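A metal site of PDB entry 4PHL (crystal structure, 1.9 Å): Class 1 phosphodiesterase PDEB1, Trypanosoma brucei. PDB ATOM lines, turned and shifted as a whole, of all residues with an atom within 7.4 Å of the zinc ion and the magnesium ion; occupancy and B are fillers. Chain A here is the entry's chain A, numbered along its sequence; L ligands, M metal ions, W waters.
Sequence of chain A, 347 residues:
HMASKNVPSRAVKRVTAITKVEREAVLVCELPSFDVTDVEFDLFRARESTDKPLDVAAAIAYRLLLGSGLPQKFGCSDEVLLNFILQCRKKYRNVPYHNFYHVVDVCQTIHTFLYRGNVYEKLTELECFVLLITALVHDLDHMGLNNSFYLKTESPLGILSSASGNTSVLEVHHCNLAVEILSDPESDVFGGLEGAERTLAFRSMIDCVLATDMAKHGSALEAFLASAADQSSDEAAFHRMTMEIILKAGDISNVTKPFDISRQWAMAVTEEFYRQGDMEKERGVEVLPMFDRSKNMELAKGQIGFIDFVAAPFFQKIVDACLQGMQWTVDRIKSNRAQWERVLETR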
ATOM      1  N   TYR A  97       7.217 -23.952  -4.306  1.00  0.00           N
ATOM      2  CA  TYR A  97       6.521 -22.656  -4.312  1.00  0.00           C
ATOM      3  C   TYR A  97       6.321 -22.100  -2.912  1.00  0.00           C
ATOM      4  O   TYR A  97       6.736 -20.971  -2.634  1.00  0.00           O
ATOM      5  CB  TYR A  97       5.160 -22.747  -5.026  1.00  0.00           C
ATOM      6  CG  TYR A  97       4.445 -21.412  -5.065  1.00  0.00           C
ATOM      7  CD1 TYR A  97       4.825 -20.403  -5.952  1.00  0.00           C
ATOM      8  CD2 TYR A  97       3.424 -21.128  -4.178  1.00  0.00           C
ATOM      9  CE1 TYR A  97       4.172 -19.163  -5.977  1.00  0.00           C
ATOM     10  CE2 TYR A  97       2.763 -19.883  -4.186  1.00  0.00           C
ATOM     11  CZ  TYR A  97       3.145 -18.910  -5.084  1.00  0.00           C
ATOM     12  OH  TYR A  97       2.473 -17.683  -5.079  1.00  0.00           O
ATOM     13  N   HIS A  98       5.697 -22.870  -2.033  1.00  0.00           N
ATOM     14  CA  HIS A  98       5.398 -22.355  -0.690  1.00  0.00           C
ATOM     15  C   HIS A  98       6.623 -22.414   0.237  1.00  0.00           C
ATOM     16  O   HIS A  98       6.601 -23.037   1.288  1.00  0.00           O
ATOM     17  CB  HIS A  98       4.183 -23.096  -0.091  1.00  0.00           C
ATOM     18  CG  HIS A  98       2.888 -22.699  -0.721  1.00  0.00           C
ATOM     19  ND1 HIS A  98       2.245 -23.486  -1.666  1.00  0.00           N
ATOM     20  CD2 HIS A  98       2.141 -21.568  -0.606  1.00  0.00           C
ATOM     21  CE1 HIS A  98       1.146 -22.868  -2.065  1.00  0.00           C
ATOM     22  NE2 HIS A  98       1.059 -21.705  -1.437  1.00  0.00           N
ATOM     23  N   HIS A 102       8.529 -17.252  -1.306  1.00  0.00           N
ATOM     24  CA  HIS A 102       7.137 -16.831  -1.459  1.00  0.00           C
ATOM     25  C   HIS A 102       6.720 -15.869  -0.350  1.00  0.00           C
ATOM     26  O   HIS A 102       6.078 -14.864  -0.641  1.00  0.00           O
ATOM     27  CB  HIS A 102       6.180 -18.051  -1.484  1.00  0.00           C
ATOM     28  CG  HIS A 102       4.726 -17.722  -1.258  1.00  0.00           C
ATOM     29  ND1 HIS A 102       3.979 -16.971  -2.153  1.00  0.00           N
ATOM     30  CD2 HIS A 102       3.874 -18.066  -0.265  1.00  0.00           C
ATOM     31  CE1 HIS A 102       2.741 -16.856  -1.697  1.00  0.00           C
ATOM     32  NE2 HIS A 102       2.638 -17.519  -0.556  1.00  0.00           N
ATOM     33  N   VAL A 103       7.045 -16.159   0.900  1.00  0.00           N
ATOM     34  CA  VAL A 103       6.548 -15.260   1.946  1.00  0.00           C
ATOM     35  C   VAL A 103       7.357 -13.937   1.971  1.00  0.00           C
ATOM     36  O   VAL A 103       6.800 -12.899   2.333  1.00  0.00           O
ATOM     37  CB  VAL A 103       6.553 -15.951   3.331  1.00  0.00           C
ATOM     38  CG1 VAL A 103       5.745 -17.265   3.269  1.00  0.00           C
ATOM     39  CG2 VAL A 103       7.975 -16.202   3.883  1.00  0.00           C
ATOM     40  N   VAL A 106       5.654 -12.061  -0.579  1.00  0.00           N
ATOM     41  CA  VAL A 106       4.344 -11.534  -0.173  1.00  0.00           C
ATOM     42  C   VAL A 106       4.581 -10.282   0.696  1.00  0.00           C
ATOM     43  O   VAL A 106       3.849  -9.305   0.590  1.00  0.00           O
ATOM     44  CB  VAL A 106       3.515 -12.597   0.574  1.00  0.00           C
ATOM     45  CG1 VAL A 106       2.303 -11.945   1.264  1.00  0.00           C
ATOM     46  CG2 VAL A 106       3.035 -13.660  -0.413  1.00  0.00           C
ATOM     47  N   ALA A 135       2.826 -11.443   6.785  1.00  0.00           N
ATOM     48  CA  ALA A 135       3.336 -11.993   5.519  1.00  0.00           C
ATOM     49  C   ALA A 135       4.408 -13.098   5.736  1.00  0.00           C
ATOM     50  O   ALA A 135       4.409 -14.130   5.049  1.00  0.00           O
ATOM     51  CB  ALA A 135       3.921 -10.887   4.665  1.00  0.00           C
ATOM     52  N   HIS A 138       2.760 -16.474   7.263  1.00  0.00           N
ATOM     53  CA  HIS A 138       1.443 -16.946   6.841  1.00  0.00           C
ATOM     54  C   HIS A 138       1.438 -18.336   6.172  1.00  0.00           C
ATOM     55  O   HIS A 138       0.373 -18.901   5.980  1.00  0.00           O
ATOM     56  CB  HIS A 138       0.781 -15.917   5.922  1.00  0.00           C
ATOM     57  CG  HIS A 138       1.152 -16.066   4.475  1.00  0.00           C
ATOM     58  ND1 HIS A 138       2.277 -15.496   3.933  1.00  0.00           N
ATOM     59  CD2 HIS A 138       0.522 -16.713   3.468  1.00  0.00           C
ATOM     60  CE1 HIS A 138       2.337 -15.793   2.638  1.00  0.00           C
ATOM     61  NE2 HIS A 138       1.282 -16.517   2.328  1.00  0.00           N
ATOM     62  N   ASP A 139       2.605 -18.886   5.832  1.00  0.00           N
ATOM     63  CA  ASP A 139       2.655 -20.230   5.245  1.00  0.00           C
ATOM     64  C   ASP A 139       3.626 -21.169   5.972  1.00  0.00           C
ATOM     65  O   ASP A 139       4.083 -22.151   5.383  1.00  0.00           O
ATOM     66  CB  ASP A 139       3.056 -20.166   3.756  1.00  0.00           C
ATOM     67  CG  ASP A 139       1.865 -19.915   2.819  1.00  0.00           C
ATOM     68  OD1 ASP A 139       0.732 -20.354   3.108  1.00  0.00           O
ATOM     69  OD2 ASP A 139       2.096 -19.309   1.780  1.00  0.00           O
ATOM     70  N   LEU A 140       3.933 -20.878   7.237  1.00  0.00           N
ATOM     71  CA  LEU A 140       4.978 -21.619   7.959  1.00  0.00           C
ATOM     72  C   LEU A 140       4.844 -23.135   7.857  1.00  0.00           C
ATOM     73  O   LEU A 140       3.771 -23.685   8.118  1.00  0.00           O
ATOM     74  CB  LEU A 140       4.981 -21.223   9.449  1.00  0.00           C
ATOM     75  CG  LEU A 140       5.583 -19.846   9.797  1.00  0.00           C
ATOM     76  CD1 LEU A 140       5.193 -19.478  11.234  1.00  0.00           C
ATOM     77  CD2 LEU A 140       7.113 -19.833   9.636  1.00  0.00           C
ATOM     78  N   HIS A 142       4.705 -25.085   5.377  1.00  0.00           N
ATOM     79  CA  HIS A 142       3.974 -25.642   4.235  1.00  0.00           C
ATOM     80  C   HIS A 142       4.759 -26.826   3.614  1.00  0.00           C
ATOM     81  O   HIS A 142       5.970 -26.709   3.360  1.00  0.00           O
ATOM     82  CB  HIS A 142       3.744 -24.576   3.177  1.00  0.00           C
ATOM     83  CG  HIS A 142       2.543 -24.820   2.323  1.00  0.00           C
ATOM     84  ND1 HIS A 142       2.434 -25.902   1.472  1.00  0.00           N
ATOM     85  CD2 HIS A 142       1.405 -24.101   2.150  1.00  0.00           C
ATOM     86  CE1 HIS A 142       1.270 -25.856   0.843  1.00  0.00           C
ATOM     87  NE2 HIS A 142       0.642 -24.761   1.234  1.00  0.00           N
ATOM     88  N   LEU A 170      -4.032 -26.364   7.023  1.00  0.00           N
ATOM     89  CA  LEU A 170      -2.762 -25.653   6.886  1.00  0.00           C
ATOM     90  C   LEU A 170      -2.722 -24.358   7.694  1.00  0.00           C
ATOM     91  O   LEU A 170      -1.758 -24.085   8.403  1.00  0.00           O
ATOM     92  CB  LEU A 170      -2.492 -25.325   5.425  1.00  0.00           C
ATOM     93  CG  LEU A 170      -1.975 -26.447   4.552  1.00  0.00           C
ATOM     94  CD1 LEU A 170      -2.021 -25.977   3.101  1.00  0.00           C
ATOM     95  CD2 LEU A 170      -0.554 -26.738   4.966  1.00  0.00           C
ATOM     96  N   GLU A 171      -3.774 -23.553   7.559  1.00  0.00           N
ATOM     97  CA  GLU A 171      -3.720 -22.194   8.099  1.00  0.00           C
ATOM     98  C   GLU A 171      -3.695 -22.220   9.630  1.00  0.00           C
ATOM     99  O   GLU A 171      -3.020 -21.416  10.262  1.00  0.00           O
ATOM    100  CB  GLU A 171      -4.896 -21.357   7.560  1.00  0.00           C
ATOM    101  CG  GLU A 171      -4.763 -21.037   6.058  1.00  0.00           C
ATOM    102  CD  GLU A 171      -5.097 -22.229   5.146  1.00  0.00           C
ATOM    103  OE1 GLU A 171      -5.793 -23.173   5.597  1.00  0.00           O
ATOM    104  OE2 GLU A 171      -4.696 -22.195   3.956  1.00  0.00           O
ATOM    105  N   HIS A 174      -0.123 -22.999  10.385  1.00  0.00           N
ATOM    106  CA  HIS A 174       0.754 -21.833  10.285  1.00  0.00           C
ATOM    107  C   HIS A 174       0.609 -20.950  11.538  1.00  0.00           C
ATOM    108  O   HIS A 174       1.602 -20.453  12.063  1.00  0.00           O
ATOM    109  CB  HIS A 174       0.480 -20.983   9.031  1.00  0.00           C
ATOM    110  CG  HIS A 174       0.401 -21.777   7.758  1.00  0.00           C
ATOM    111  ND1 HIS A 174       1.279 -22.798   7.441  1.00  0.00           N
ATOM    112  CD2 HIS A 174      -0.464 -21.700   6.721  1.00  0.00           C
ATOM    113  CE1 HIS A 174       0.970 -23.287   6.250  1.00  0.00           C
ATOM    114  NE2 HIS A 174      -0.094 -22.650   5.804  1.00  0.00           N
ATOM    115  N   VAL A 209      -4.102 -14.723   8.743  1.00  0.00           N
ATOM    116  CA  VAL A 209      -3.627 -16.020   8.251  1.00  0.00           C
ATOM    117  C   VAL A 209      -4.785 -16.983   7.933  1.00  0.00           C
ATOM    118  O   VAL A 209      -4.818 -17.624   6.864  1.00  0.00           O
ATOM    119  CB  VAL A 209      -2.655 -16.688   9.250  1.00  0.00           C
ATOM    120  CG1 VAL A 209      -2.212 -18.049   8.740  1.00  0.00           C
ATOM    121  CG2 VAL A 209      -1.424 -15.799   9.407  1.00  0.00           C
ATOM    122  N   THR A 212      -6.429 -16.627   4.602  1.00  0.00           N
ATOM    123  CA  THR A 212      -5.738 -16.950   3.352  1.00  0.00           C
ATOM    124  C   THR A 212      -6.184 -18.293   2.758  1.00  0.00           C
ATOM    125  O   THR A 212      -5.837 -18.611   1.617  1.00  0.00           O
ATOM    126  CB  THR A 212      -4.190 -16.972   3.500  1.00  0.00           C
ATOM    127  OG1 THR A 212      -3.767 -17.895   4.513  1.00  0.00           O
ATOM    128  CG2 THR A 212      -3.678 -15.593   3.849  1.00  0.00           C
ATOM    129  N   ASP A 213      -6.954 -19.070   3.511  1.00  0.00           N
ATOM    130  CA  ASP A 213      -7.552 -20.309   2.984  1.00  0.00           C
ATOM    131  C   ASP A 213      -8.466 -19.945   1.809  1.00  0.00           C
ATOM    132  O   ASP A 213      -9.440 -19.235   2.006  1.00  0.00           O
ATOM    133  CB  ASP A 213      -8.330 -21.026   4.108  1.00  0.00           C
ATOM    134  CG  ASP A 213      -8.933 -22.366   3.656  1.00  0.00           C
ATOM    135  OD1 ASP A 213      -8.854 -22.702   2.451  1.00  0.00           O
ATOM    136  OD2 ASP A 213      -9.504 -23.068   4.528  1.00  0.00           O
ATOM    137  N   MET A 214      -8.158 -20.407   0.605  1.00  0.00           N
ATOM    138  CA  MET A 214      -8.964 -20.041  -0.565  1.00  0.00           C
ATOM    139  C   MET A 214     -10.392 -20.606  -0.539  1.00  0.00           C
ATOM    140  O   MET A 214     -11.241 -20.191  -1.330  1.00  0.00           O
ATOM    141  CB  MET A 214      -8.270 -20.460  -1.876  1.00  0.00           C
ATOM    142  CG  MET A 214      -7.055 -19.578  -2.232  1.00  0.00           C
ATOM    143  SD  MET A 214      -7.475 -17.840  -2.568  1.00  0.00           S
ATOM    144  CE  MET A 214      -8.025 -17.972  -4.265  1.00  0.00           C
ATOM    145  N   LEU A 247      -3.553  -9.050   2.780  1.00  0.00           N
ATOM    146  CA  LEU A 247      -2.761 -10.276   2.833  1.00  0.00           C
ATOM    147  C   LEU A 247      -3.225 -11.244   1.719  1.00  0.00           C
ATOM    148  O   LEU A 247      -2.387 -11.826   1.036  1.00  0.00           O
ATOM    149  CB  LEU A 247      -2.855 -10.957   4.214  1.00  0.00           C
ATOM    150  CG  LEU A 247      -2.062 -12.278   4.297  1.00  0.00           C
ATOM    151  CD1 LEU A 247      -0.588 -12.068   3.990  1.00  0.00           C
ATOM    152  CD2 LEU A 247      -2.217 -13.020   5.646  1.00  0.00           C
ATOM    153  N   GLY A 250      -1.732  -9.930  -1.511  1.00  0.00           N
ATOM    154  CA  GLY A 250      -0.317 -10.234  -1.626  1.00  0.00           C
ATOM    155  C   GLY A 250      -0.104 -11.677  -2.035  1.00  0.00           C
ATOM    156  O   GLY A 250       0.747 -11.998  -2.887  1.00  0.00           O
ATOM    157  N   ASP A 251      -0.894 -12.550  -1.422  1.00  0.00           N
ATOM    158  CA  ASP A 251      -0.833 -13.994  -1.672  1.00  0.00           C
ATOM    159  C   ASP A 251      -1.155 -14.357  -3.129  1.00  0.00           C
ATOM    160  O   ASP A 251      -0.552 -15.278  -3.679  1.00  0.00           O
ATOM    161  CB  ASP A 251      -1.803 -14.713  -0.732  1.00  0.00           C
ATOM    162  CG  ASP A 251      -1.306 -16.084  -0.291  1.00  0.00           C
ATOM    163  OD1 ASP A 251      -0.100 -16.405  -0.455  1.00  0.00           O
ATOM    164  OD2 ASP A 251      -2.152 -16.830   0.244  1.00  0.00           O
ATOM    165  N   ILE A 252      -2.111 -13.646  -3.754  1.00  0.00           N
ATOM    166  CA  ILE A 252      -2.418 -13.935  -5.158  1.00  0.00           C
ATOM    167  C   ILE A 252      -1.834 -12.921  -6.145  1.00  0.00           C
ATOM    168  O   ILE A 252      -2.345 -12.787  -7.274  1.00  0.00           O
ATOM    169  CB  ILE A 252      -3.939 -13.990  -5.464  1.00  0.00           C
ATOM    170  CG1 ILE A 252      -4.665 -12.732  -5.011  1.00  0.00           C
ATOM    171  CG2 ILE A 252      -4.599 -15.144  -4.838  1.00  0.00           C
ATOM    172  CD1 ILE A 252      -6.150 -12.883  -5.212  1.00  0.00           C
HETATM  173 CL1  LIG L   1      -1.935 -22.384  -4.117  1.00  0.00          CL
HETATM  174  C1  LIG L   1      -2.679 -21.210  -3.069  1.00  0.00           C
HETATM  175  C2  LIG L   1      -3.220 -21.603  -1.855  1.00  0.00           C
HETATM  176  N1  LIG L   1      -3.788 -20.677  -1.037  1.00  0.00           N
HETATM  177  C3  LIG L   1      -3.835 -19.362  -1.407  1.00  0.00           C
HETATM  178  C4  LIG L   1      -3.288 -18.982  -2.626  1.00  0.00           C
HETATM  179 CL2  LIG L   1      -3.334 -17.322  -3.105  1.00  0.00          CL
HETATM  180  C5  LIG L   1      -2.721 -19.898  -3.448  1.00  0.00           C
HETATM  181  N2  LIG L   1      -2.137 -19.518  -4.707  1.00  0.00           N
HETATM  182  C6  LIG L   1      -2.730 -19.868  -5.964  1.00  0.00           C
HETATM  183  O1  LIG L   1      -3.760 -20.511  -6.056  1.00  0.00           O
HETATM  184  C7  LIG L   1      -1.977 -19.459  -7.220  1.00  0.00           C
HETATM  185  C8  LIG L   1      -0.982 -18.507  -7.150  1.00  0.00           C
HETATM  186  C9  LIG L   1      -0.284 -18.164  -8.308  1.00  0.00           C
HETATM  187  C10 LIG L   1      -0.587 -18.795  -9.510  1.00  0.00           C
HETATM  188  O2  LIG L   1       0.137 -18.436 -10.661  1.00  0.00           O
HETATM  189  C11 LIG L   1       1.454 -17.998 -10.331  1.00  0.00           C
HETATM  190  C12 LIG L   1      -1.576 -19.768  -9.582  1.00  0.00           C
HETATM  191  C13 LIG L   1      -2.274 -20.111  -8.423  1.00  0.00           C
HETATM  192  O3  LIG L   1      -1.867 -20.399 -10.812  1.00  0.00           O
HETATM  193  C14 LIG L   1      -2.364 -21.745 -10.612  1.00  0.00           C
HETATM  194  C15 LIG L   1      -1.482 -22.727 -11.378  1.00  0.00           C
HETATM  195  C16 LIG L   1      -2.357 -23.147 -12.689  1.00  0.00           C
HETATM  196  C17 LIG L   1      -3.729 -22.297 -12.496  1.00  0.00           C
HETATM  197  C18 LIG L   1      -3.679 -21.820 -11.147  1.00  0.00           C
HETATM  198 ZN    ZN M   1       1.057 -17.816   0.626  1.00  0.00          ZN
HETATM  199 MG    MG M   2      -1.325 -20.384   2.549  1.00  0.00          MG
HETATM  200  O   HOH W   1      -1.669 -22.255   3.497  1.00  0.00           O
HETATM  201  O   HOH W   2      -0.702 -18.822   1.176  1.00  0.00           O
HETATM  202  O   HOH W   3      -0.887 -21.445   0.755  1.00  0.00           O
HETATM  203  O   HOH W   4      -0.022 -19.198  -1.123  1.00  0.00           O
HETATM  204  O   HOH W   5      -3.455 -20.525   2.325  1.00  0.00           O
HETATM  205  O   HOH W   6      -1.669 -19.451   4.406  1.00  0.00           O
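Within 4 Å of the zinc ion: His 102, His 138, Asp 139 and Asp 251.
The nearest printed residue that does not touch the zinc ion is His 98 (4.1 Å).
The zinc ion is bound by NE2 of His 102, water W2, OD1 of Asp 251, NE2 of His 138, OD2 of Asp 139 and water W4.
Water W4 bridges NE2 of His 98 (2.7 Å) and OD2 of Asp 251 (3.5 Å).
Water W3 bridges NE2 of His 98 (2.9 Å) and N1 of the ligand (3.5 Å).
Water W6 lies within hydrogen-bond range of OG1 of Thr 212 (2.6 Å) and O of His 138 (2.6 Å).
Water W1 lies within hydrogen-bond range of a ring nitrogen (NE2) of His 174 (2.8 Å) and the side-chain carboxylate of Glu 171 (3.1 Å).
Water W6 binds the magnesium ion (2.1 Å).
Water W1 binds the magnesium ion (2.1 Å).
Water W3 binds the magnesium ion (2.1 Å).
OD1 of Asp 139 binds the magnesium ion (2.1 Å).
The magnesium ion is bound by water W5.
The magnesium ion is bound by water W2 (2.2 Å).
One residue has an atom within 4 Å of the magnesium ion: Asp 139.
The nearest printed residue that does not touch the magnesium ion is Thr 212 (4.002 Å).
A ring nitrogen (ND1) of His 102 is in hydrogen-bond range of the side-chain hydroxyl (OH) of Tyr 97.
A ring nitrogen (ND1) of His 138 is in hydrogen-bond range of the backbone carbonyl oxygen (O) of Ala 135 (2.8 Å).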
